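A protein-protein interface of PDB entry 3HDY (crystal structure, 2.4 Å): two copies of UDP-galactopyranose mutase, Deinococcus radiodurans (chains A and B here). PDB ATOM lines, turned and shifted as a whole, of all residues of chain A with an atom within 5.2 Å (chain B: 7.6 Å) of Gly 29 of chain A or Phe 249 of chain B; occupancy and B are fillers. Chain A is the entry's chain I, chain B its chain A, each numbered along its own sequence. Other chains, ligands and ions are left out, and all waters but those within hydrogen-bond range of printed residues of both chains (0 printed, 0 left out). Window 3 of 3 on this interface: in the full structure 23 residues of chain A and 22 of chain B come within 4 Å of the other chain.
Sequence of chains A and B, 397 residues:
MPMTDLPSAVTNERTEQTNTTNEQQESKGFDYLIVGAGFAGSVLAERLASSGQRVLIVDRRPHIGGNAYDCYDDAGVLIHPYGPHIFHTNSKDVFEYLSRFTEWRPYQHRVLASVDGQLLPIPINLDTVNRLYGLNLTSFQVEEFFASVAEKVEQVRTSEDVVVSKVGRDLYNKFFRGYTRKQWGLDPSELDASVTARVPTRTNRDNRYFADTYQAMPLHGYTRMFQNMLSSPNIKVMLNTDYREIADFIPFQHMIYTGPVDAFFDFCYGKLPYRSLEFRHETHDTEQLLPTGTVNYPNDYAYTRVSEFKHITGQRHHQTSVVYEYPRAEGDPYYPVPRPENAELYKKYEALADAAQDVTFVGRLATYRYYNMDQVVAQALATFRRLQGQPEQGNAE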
ATOM      1  N   GLY A  29     -17.498 -14.442   0.492  1.00  0.00           N
ATOM      2  CA  GLY A  29     -17.508 -13.027   0.165  1.00  0.00           C
ATOM      3  C   GLY A  29     -17.806 -12.130   1.355  1.00  0.00           C
ATOM      4  O   GLY A  29     -17.498 -12.472   2.499  1.00  0.00           O
ATOM      5  N   PHE A  30     -18.409 -10.976   1.079  1.00  0.00           N
ATOM      6  CA  PHE A  30     -18.723  -9.998   2.113  1.00  0.00           C
ATOM      7  C   PHE A  30     -20.189  -9.591   2.053  1.00  0.00           C
ATOM      8  O   PHE A  30     -20.839  -9.727   1.018  1.00  0.00           O
ATOM      9  CB  PHE A  30     -17.855  -8.746   1.952  1.00  0.00           C
ATOM     10  CG  PHE A  30     -16.379  -9.026   1.920  1.00  0.00           C
ATOM     11  CD1 PHE A  30     -15.762  -9.419   0.744  1.00  0.00           C
ATOM     12  CD2 PHE A  30     -15.608  -8.886   3.061  1.00  0.00           C
ATOM     13  CE1 PHE A  30     -14.406  -9.675   0.707  1.00  0.00           C
ATOM     14  CE2 PHE A  30     -14.245  -9.141   3.032  1.00  0.00           C
ATOM     15  CZ  PHE A  30     -13.645  -9.536   1.852  1.00  0.00           C
ATOM     16  N   ASP A  31     -20.698  -9.076   3.168  1.00  0.00           N
ATOM     17  CA  ASP A  31     -22.047  -8.526   3.210  1.00  0.00           C
ATOM     18  C   ASP A  31     -22.048  -7.103   2.653  1.00  0.00           C
ATOM     19  O   ASP A  31     -23.033  -6.659   2.058  1.00  0.00           O
ATOM     20  CB  ASP A  31     -22.583  -8.525   4.642  1.00  0.00           C
ATOM     21  CG  ASP A  31     -22.498  -9.890   5.298  1.00  0.00           C
ATOM     22  OD1 ASP A  31     -22.152 -10.867   4.600  1.00  0.00           O
ATOM     23  OD2 ASP A  31     -22.776  -9.989   6.513  1.00  0.00           O
ATOM     24  N   ARG A  54     -19.994  -8.975   7.653  1.00  0.00           N
ATOM     25  CA  ARG A  54     -18.628  -9.055   7.145  1.00  0.00           C
ATOM     26  C   ARG A  54     -18.378  -7.945   6.135  1.00  0.00           C
ATOM     27  O   ARG A  54     -18.938  -7.944   5.037  1.00  0.00           O
ATOM     28  CB  ARG A  54     -18.322 -10.421   6.530  1.00  0.00           C
ATOM     29  CG  ARG A  54     -17.747 -11.418   7.521  1.00  0.00           C
ATOM     30  CD  ARG A  54     -16.499 -12.084   6.961  1.00  0.00           C
ATOM     31  NE  ARG A  54     -16.800 -13.015   5.877  1.00  0.00           N
ATOM     32  CZ  ARG A  54     -15.889 -13.506   5.040  1.00  0.00           C
ATOM     33  NH1 ARG A  54     -14.616 -13.146   5.155  1.00  0.00           N
ATOM     34  NH2 ARG A  54     -16.254 -14.354   4.084  1.00  0.00           N
ATOM     35  N   PHE A 249     -14.699  -9.250  -9.405  1.00  0.00           N
ATOM     36  CA  PHE A 249     -14.411 -10.597  -8.913  1.00  0.00           C
ATOM     37  C   PHE A 249     -14.413 -10.743  -7.389  1.00  0.00           C
ATOM     38  O   PHE A 249     -13.820 -11.678  -6.856  1.00  0.00           O
ATOM     39  CB  PHE A 249     -13.090 -11.119  -9.488  1.00  0.00           C
ATOM     40  CG  PHE A 249     -11.919 -10.221  -9.226  1.00  0.00           C
ATOM     41  CD1 PHE A 249     -11.246  -9.619 -10.274  1.00  0.00           C
ATOM     42  CD2 PHE A 249     -11.493  -9.972  -7.929  1.00  0.00           C
ATOM     43  CE1 PHE A 249     -10.166  -8.789 -10.037  1.00  0.00           C
ATOM     44  CE2 PHE A 249     -10.416  -9.142  -7.685  1.00  0.00           C
ATOM     45  CZ  PHE A 249      -9.751  -8.551  -8.741  1.00  0.00           C
ATOM     46  N   ILE A 250     -15.079  -9.828  -6.691  1.00  0.00           N
ATOM     47  CA  ILE A 250     -15.223  -9.949  -5.243  1.00  0.00           C
ATOM     48  C   ILE A 250     -16.688  -9.986  -4.824  1.00  0.00           C
ATOM     49  O   ILE A 250     -17.433  -9.036  -5.054  1.00  0.00           O
ATOM     50  CB  ILE A 250     -14.500  -8.820  -4.484  1.00  0.00           C
ATOM     51  CG1 ILE A 250     -12.985  -9.014  -4.562  1.00  0.00           C
ATOM     52  CG2 ILE A 250     -14.942  -8.789  -3.030  1.00  0.00           C
ATOM     53  CD1 ILE A 250     -12.213  -8.214  -3.533  1.00  0.00           C
ATOM     54  N   PRO A 251     -17.101 -11.097  -4.201  1.00  0.00           N
ATOM     55  CA  PRO A 251     -18.482 -11.346  -3.770  1.00  0.00           C
ATOM     56  C   PRO A 251     -18.935 -10.424  -2.644  1.00  0.00           C
ATOM     57  O   PRO A 251     -18.427 -10.521  -1.529  1.00  0.00           O
ATOM     58  CB  PRO A 251     -18.432 -12.790  -3.255  1.00  0.00           C
ATOM     59  CG  PRO A 251     -17.195 -13.377  -3.852  1.00  0.00           C
ATOM     60  CD  PRO A 251     -16.228 -12.253  -3.949  1.00  0.00           C
ATOM     61  N   SER B  27     -12.453 -16.680 -13.197  1.00  0.00           N
ATOM     62  CA  SER B  27     -11.632 -15.493 -13.420  1.00  0.00           C
ATOM     63  C   SER B  27     -10.133 -15.777 -13.355  1.00  0.00           C
ATOM     64  O   SER B  27      -9.698 -16.753 -12.746  1.00  0.00           O
ATOM     65  CB  SER B  27     -12.003 -14.400 -12.408  1.00  0.00           C
ATOM     66  OG  SER B  27     -11.187 -13.250 -12.562  1.00  0.00           O
ATOM     67  N   MET B 238      -3.935  -5.332   1.196  1.00  0.00           N
ATOM     68  CA  MET B 238      -5.052  -5.759   2.030  1.00  0.00           C
ATOM     69  C   MET B 238      -4.602  -6.040   3.463  1.00  0.00           C
ATOM     70  O   MET B 238      -3.740  -6.888   3.701  1.00  0.00           O
ATOM     71  CB  MET B 238      -5.737  -6.989   1.428  1.00  0.00           C
ATOM     72  CG  MET B 238      -7.147  -7.213   1.946  1.00  0.00           C
ATOM     73  SD  MET B 238      -8.047  -8.460   1.007  1.00  0.00           S
ATOM     74  CE  MET B 238      -9.685  -8.277   1.704  1.00  0.00           C
ATOM     75  N   THR B 241      -6.265  -9.147   7.361  1.00  0.00           N
ATOM     76  CA  THR B 241      -6.859 -10.225   6.582  1.00  0.00           C
ATOM     77  C   THR B 241      -5.951 -11.446   6.464  1.00  0.00           C
ATOM     78  O   THR B 241      -4.905 -11.387   5.821  1.00  0.00           O
ATOM     79  CB  THR B 241      -7.201  -9.739   5.160  1.00  0.00           C
ATOM     80  OG1 THR B 241      -8.030  -8.574   5.239  1.00  0.00           O
ATOM     81  CG2 THR B 241      -7.923 -10.821   4.378  1.00  0.00           C
ATOM     82  N   TYR B 243      -4.973 -14.756   4.758  1.00  0.00           N
ATOM     83  CA  TYR B 243      -5.165 -15.131   3.362  1.00  0.00           C
ATOM     84  C   TYR B 243      -6.251 -16.189   3.213  1.00  0.00           C
ATOM     85  O   TYR B 243      -6.926 -16.261   2.188  1.00  0.00           O
ATOM     86  CB  TYR B 243      -3.855 -15.606   2.724  1.00  0.00           C
ATOM     87  CG  TYR B 243      -3.463 -17.021   3.075  1.00  0.00           C
ATOM     88  CD1 TYR B 243      -3.704 -18.069   2.196  1.00  0.00           C
ATOM     89  CD2 TYR B 243      -2.842 -17.309   4.284  1.00  0.00           C
ATOM     90  CE1 TYR B 243      -3.340 -19.367   2.515  1.00  0.00           C
ATOM     91  CE2 TYR B 243      -2.476 -18.601   4.612  1.00  0.00           C
ATOM     92  CZ  TYR B 243      -2.728 -19.626   3.727  1.00  0.00           C
ATOM     93  OH  TYR B 243      -2.363 -20.911   4.053  1.00  0.00           O
ATOM     94  N   ARG B 244      -6.424 -16.998   4.251  1.00  0.00           N
ATOM     95  CA  ARG B 244      -7.453 -18.027   4.244  1.00  0.00           C
ATOM     96  C   ARG B 244      -8.862 -17.431   4.231  1.00  0.00           C
ATOM     97  O   ARG B 244      -9.810 -18.073   3.772  1.00  0.00           O
ATOM     98  CB  ARG B 244      -7.269 -18.979   5.429  1.00  0.00           C
ATOM     99  CG  ARG B 244      -6.034 -19.854   5.298  1.00  0.00           C
ATOM    100  CD  ARG B 244      -5.867 -20.761   6.497  1.00  0.00           C
ATOM    101  NE  ARG B 244      -5.548 -20.013   7.709  1.00  0.00           N
ATOM    102  CZ  ARG B 244      -4.334 -19.941   8.244  1.00  0.00           C
ATOM    103  NH1 ARG B 244      -3.318 -20.575   7.674  1.00  0.00           N
ATOM    104  NH2 ARG B 244      -4.136 -19.239   9.351  1.00  0.00           N
ATOM    105  N   GLU B 245      -8.988 -16.200   4.718  1.00  0.00           N
ATOM    106  CA  GLU B 245     -10.278 -15.513   4.735  1.00  0.00           C
ATOM    107  C   GLU B 245     -10.735 -15.065   3.348  1.00  0.00           C
ATOM    108  O   GLU B 245     -11.876 -14.634   3.183  1.00  0.00           O
ATOM    109  CB  GLU B 245     -10.235 -14.296   5.661  1.00  0.00           C
ATOM    110  CG  GLU B 245      -9.744 -14.579   7.067  1.00  0.00           C
ATOM    111  CD  GLU B 245     -10.035 -13.434   8.014  1.00  0.00           C
ATOM    112  OE1 GLU B 245      -9.078 -12.868   8.588  1.00  0.00           O
ATOM    113  OE2 GLU B 245     -11.225 -13.093   8.172  1.00  0.00           O
ATOM    114  N   ILE B 246      -9.852 -15.159   2.356  1.00  0.00           N
ATOM    115  CA  ILE B 246     -10.157 -14.641   1.022  1.00  0.00           C
ATOM    116  C   ILE B 246      -9.748 -15.576  -0.111  1.00  0.00           C
ATOM    117  O   ILE B 246     -10.277 -15.476  -1.220  1.00  0.00           O
ATOM    118  CB  ILE B 246      -9.463 -13.291   0.768  1.00  0.00           C
ATOM    119  CG1 ILE B 246      -7.953 -13.437   0.966  1.00  0.00           C
ATOM    120  CG2 ILE B 246     -10.035 -12.214   1.677  1.00  0.00           C
ATOM    121  CD1 ILE B 246      -7.135 -12.581   0.044  1.00  0.00           C
ATOM    122  N   ALA B 247      -8.802 -16.470   0.163  1.00  0.00           N
ATOM    123  CA  ALA B 247      -8.238 -17.335  -0.871  1.00  0.00           C
ATOM    124  C   ALA B 247      -9.274 -18.281  -1.479  1.00  0.00           C
ATOM    125  O   ALA B 247      -8.982 -19.011  -2.424  1.00  0.00           O
ATOM    126  CB  ALA B 247      -7.056 -18.119  -0.323  1.00  0.00           C
ATOM    127  N   ASP B 248     -10.482 -18.261  -0.931  1.00  0.00           N
ATOM    128  CA  ASP B 248     -11.566 -19.074  -1.458  1.00  0.00           C
ATOM    129  C   ASP B 248     -12.308 -18.391  -2.607  1.00  0.00           C
ATOM    130  O   ASP B 248     -12.844 -19.065  -3.484  1.00  0.00           O
ATOM    131  CB  ASP B 248     -12.554 -19.446  -0.346  1.00  0.00           C
ATOM    132  CG  ASP B 248     -12.103 -20.654   0.460  1.00  0.00           C
ATOM    133  OD1 ASP B 248     -11.213 -21.392  -0.017  1.00  0.00           O
ATOM    134  OD2 ASP B 248     -12.644 -20.869   1.569  1.00  0.00           O
ATOM    135  N   PHE B 249     -12.346 -17.060  -2.608  1.00  0.00           N
ATOM    136  CA  PHE B 249     -13.142 -16.343  -3.606  1.00  0.00           C
ATOM    137  C   PHE B 249     -12.417 -15.239  -4.386  1.00  0.00           C
ATOM    138  O   PHE B 249     -12.993 -14.632  -5.286  1.00  0.00           O
ATOM    139  CB  PHE B 249     -14.424 -15.793  -2.974  1.00  0.00           C
ATOM    140  CG  PHE B 249     -14.192 -14.999  -1.724  1.00  0.00           C
ATOM    141  CD1 PHE B 249     -14.278 -15.603  -0.483  1.00  0.00           C
ATOM    142  CD2 PHE B 249     -13.894 -13.649  -1.792  1.00  0.00           C
ATOM    143  CE1 PHE B 249     -14.070 -14.872   0.674  1.00  0.00           C
ATOM    144  CE2 PHE B 249     -13.685 -12.913  -0.642  1.00  0.00           C
ATOM    145  CZ  PHE B 249     -13.774 -13.525   0.594  1.00  0.00           C
ATOM    146  N   ILE B 250     -11.162 -14.974  -4.050  1.00  0.00           N
ATOM    147  CA  ILE B 250     -10.384 -14.014  -4.821  1.00  0.00           C
ATOM    148  C   ILE B 250      -9.489 -14.759  -5.798  1.00  0.00           C
ATOM    149  O   ILE B 250      -8.667 -15.574  -5.391  1.00  0.00           O
ATOM    150  CB  ILE B 250      -9.535 -13.102  -3.918  1.00  0.00           C
ATOM    151  CG1 ILE B 250     -10.439 -12.252  -3.027  1.00  0.00           C
ATOM    152  CG2 ILE B 250      -8.643 -12.209  -4.752  1.00  0.00           C
ATOM    153  CD1 ILE B 250      -9.681 -11.314  -2.123  1.00  0.00           C
ATOM    154  N   PRO B 251      -9.659 -14.490  -7.097  1.00  0.00           N
ATOM    155  CA  PRO B 251      -8.911 -15.187  -8.148  1.00  0.00           C
ATOM    156  C   PRO B 251      -7.436 -14.793  -8.177  1.00  0.00           C
ATOM    157  O   PRO B 251      -7.117 -13.607  -8.121  1.00  0.00           O
ATOM    158  CB  PRO B 251      -9.598 -14.717  -9.439  1.00  0.00           C
ATOM    159  CG  PRO B 251     -10.901 -14.114  -9.005  1.00  0.00           C
ATOM    160  CD  PRO B 251     -10.641 -13.548  -7.654  1.00  0.00           C
ATOM    161  N   PHE B 252      -6.551 -15.781  -8.264  1.00  0.00           N
ATOM    162  CA  PHE B 252      -5.129 -15.513  -8.448  1.00  0.00           C
ATOM    163  C   PHE B 252      -4.431 -16.651  -9.185  1.00  0.00           C
ATOM    164  O   PHE B 252      -4.783 -17.817  -9.023  1.00  0.00           O
ATOM    165  CB  PHE B 252      -4.433 -15.226  -7.110  1.00  0.00           C
ATOM    166  CG  PHE B 252      -4.587 -16.318  -6.092  1.00  0.00           C
ATOM    167  CD1 PHE B 252      -3.604 -17.282  -5.935  1.00  0.00           C
ATOM    168  CD2 PHE B 252      -5.709 -16.373  -5.280  1.00  0.00           C
ATOM    169  CE1 PHE B 252      -3.743 -18.286  -4.990  1.00  0.00           C
ATOM    170  CE2 PHE B 252      -5.853 -17.372  -4.335  1.00  0.00           C
ATOM    171  CZ  PHE B 252      -4.869 -18.330  -4.191  1.00  0.00           C
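The backbone carbonyl oxygen (O) of Phe 249 of chain A sits close to the backbone carbonyl oxygen (O) of Phe 249 of chain B, 3.4 Å away.
O of Gly 29 of chain A is in hydrogen-bond range of NH2 of Arg 54 of chain A (2.8 Å). The backbone carbonyl oxygen (O) of Pro 251 of chain A sits at hydrogen-bond distance from the backbone NH (N) of Phe 30 of chain A, 2.6 Å away. The backbone NH (N) of Asp 31 of chain A is in hydrogen-bond range of the backbone carbonyl oxygen (O) of Arg 54 of chain A, at 2.8 Å.
Among the printed residues, merely in contact across the chains: Gly 29 of chain A with Phe 249 of chain B (3.5 Å), Phe 30 of chain A with Phe 249 of chain B (3.6 Å), Arg 54 of chain A with Glu 245 of chain B (3.7 Å), Phe 249 of chain A with Pro 251 of chain B (3.7 Å) and Pro 251 of chain A with Phe 249 of chain B (3.5 Å).
Gly 29 of chain A touches just one residue of chain B: Phe 249 (3.5 Å). Of the printed residues of chain B, Phe 30 of chain A touches Phe 249 (3.6 Å). Asp 31 of chain A touches none of the printed residues of chain B. Printed residues of chain B within 4 Å of Phe 249 of chain A: Phe 249 and Pro 251. Printed residues of chain A within 4 Å of Glu 245 of chain B: Arg 54. Ala 247 of chain B touches none of the printed residues of chain A. Phe 249 of chain B touches four residues of chain A. Printed residues of chain A within 4 Å of Pro 251 of chain B: Phe 249. The nearest residue of chain B that does not touch Gly 29 of chain A is Glu 245 of chain B (6.1 Å).
Of the 13 printed residues of chain B, 3 touch a printed residue of chain A. Printed residues of chain A that touch a printed residue of chain B: Gly 29, Phe 30, Arg 54, Phe 249 and Pro 251. Among the printed residues, no Asp or Glu carboxylate lies within 4 Å of a Lys or Arg side-chain nitrogen of the other chain.
Phe 249 of chain A touches its own counterpart, Phe 249 of chain B. Phe 249 of chain A touches Pro 251 of chain B, and with the chains exchanged Pro 251 of chain A touches Phe 249 of chain B. Positions printed for both chains: 249, 250 and 251. Of the 6 pairs that touch across the chains among the printed residues, 3 have their exchanged pair printed and touching as well.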
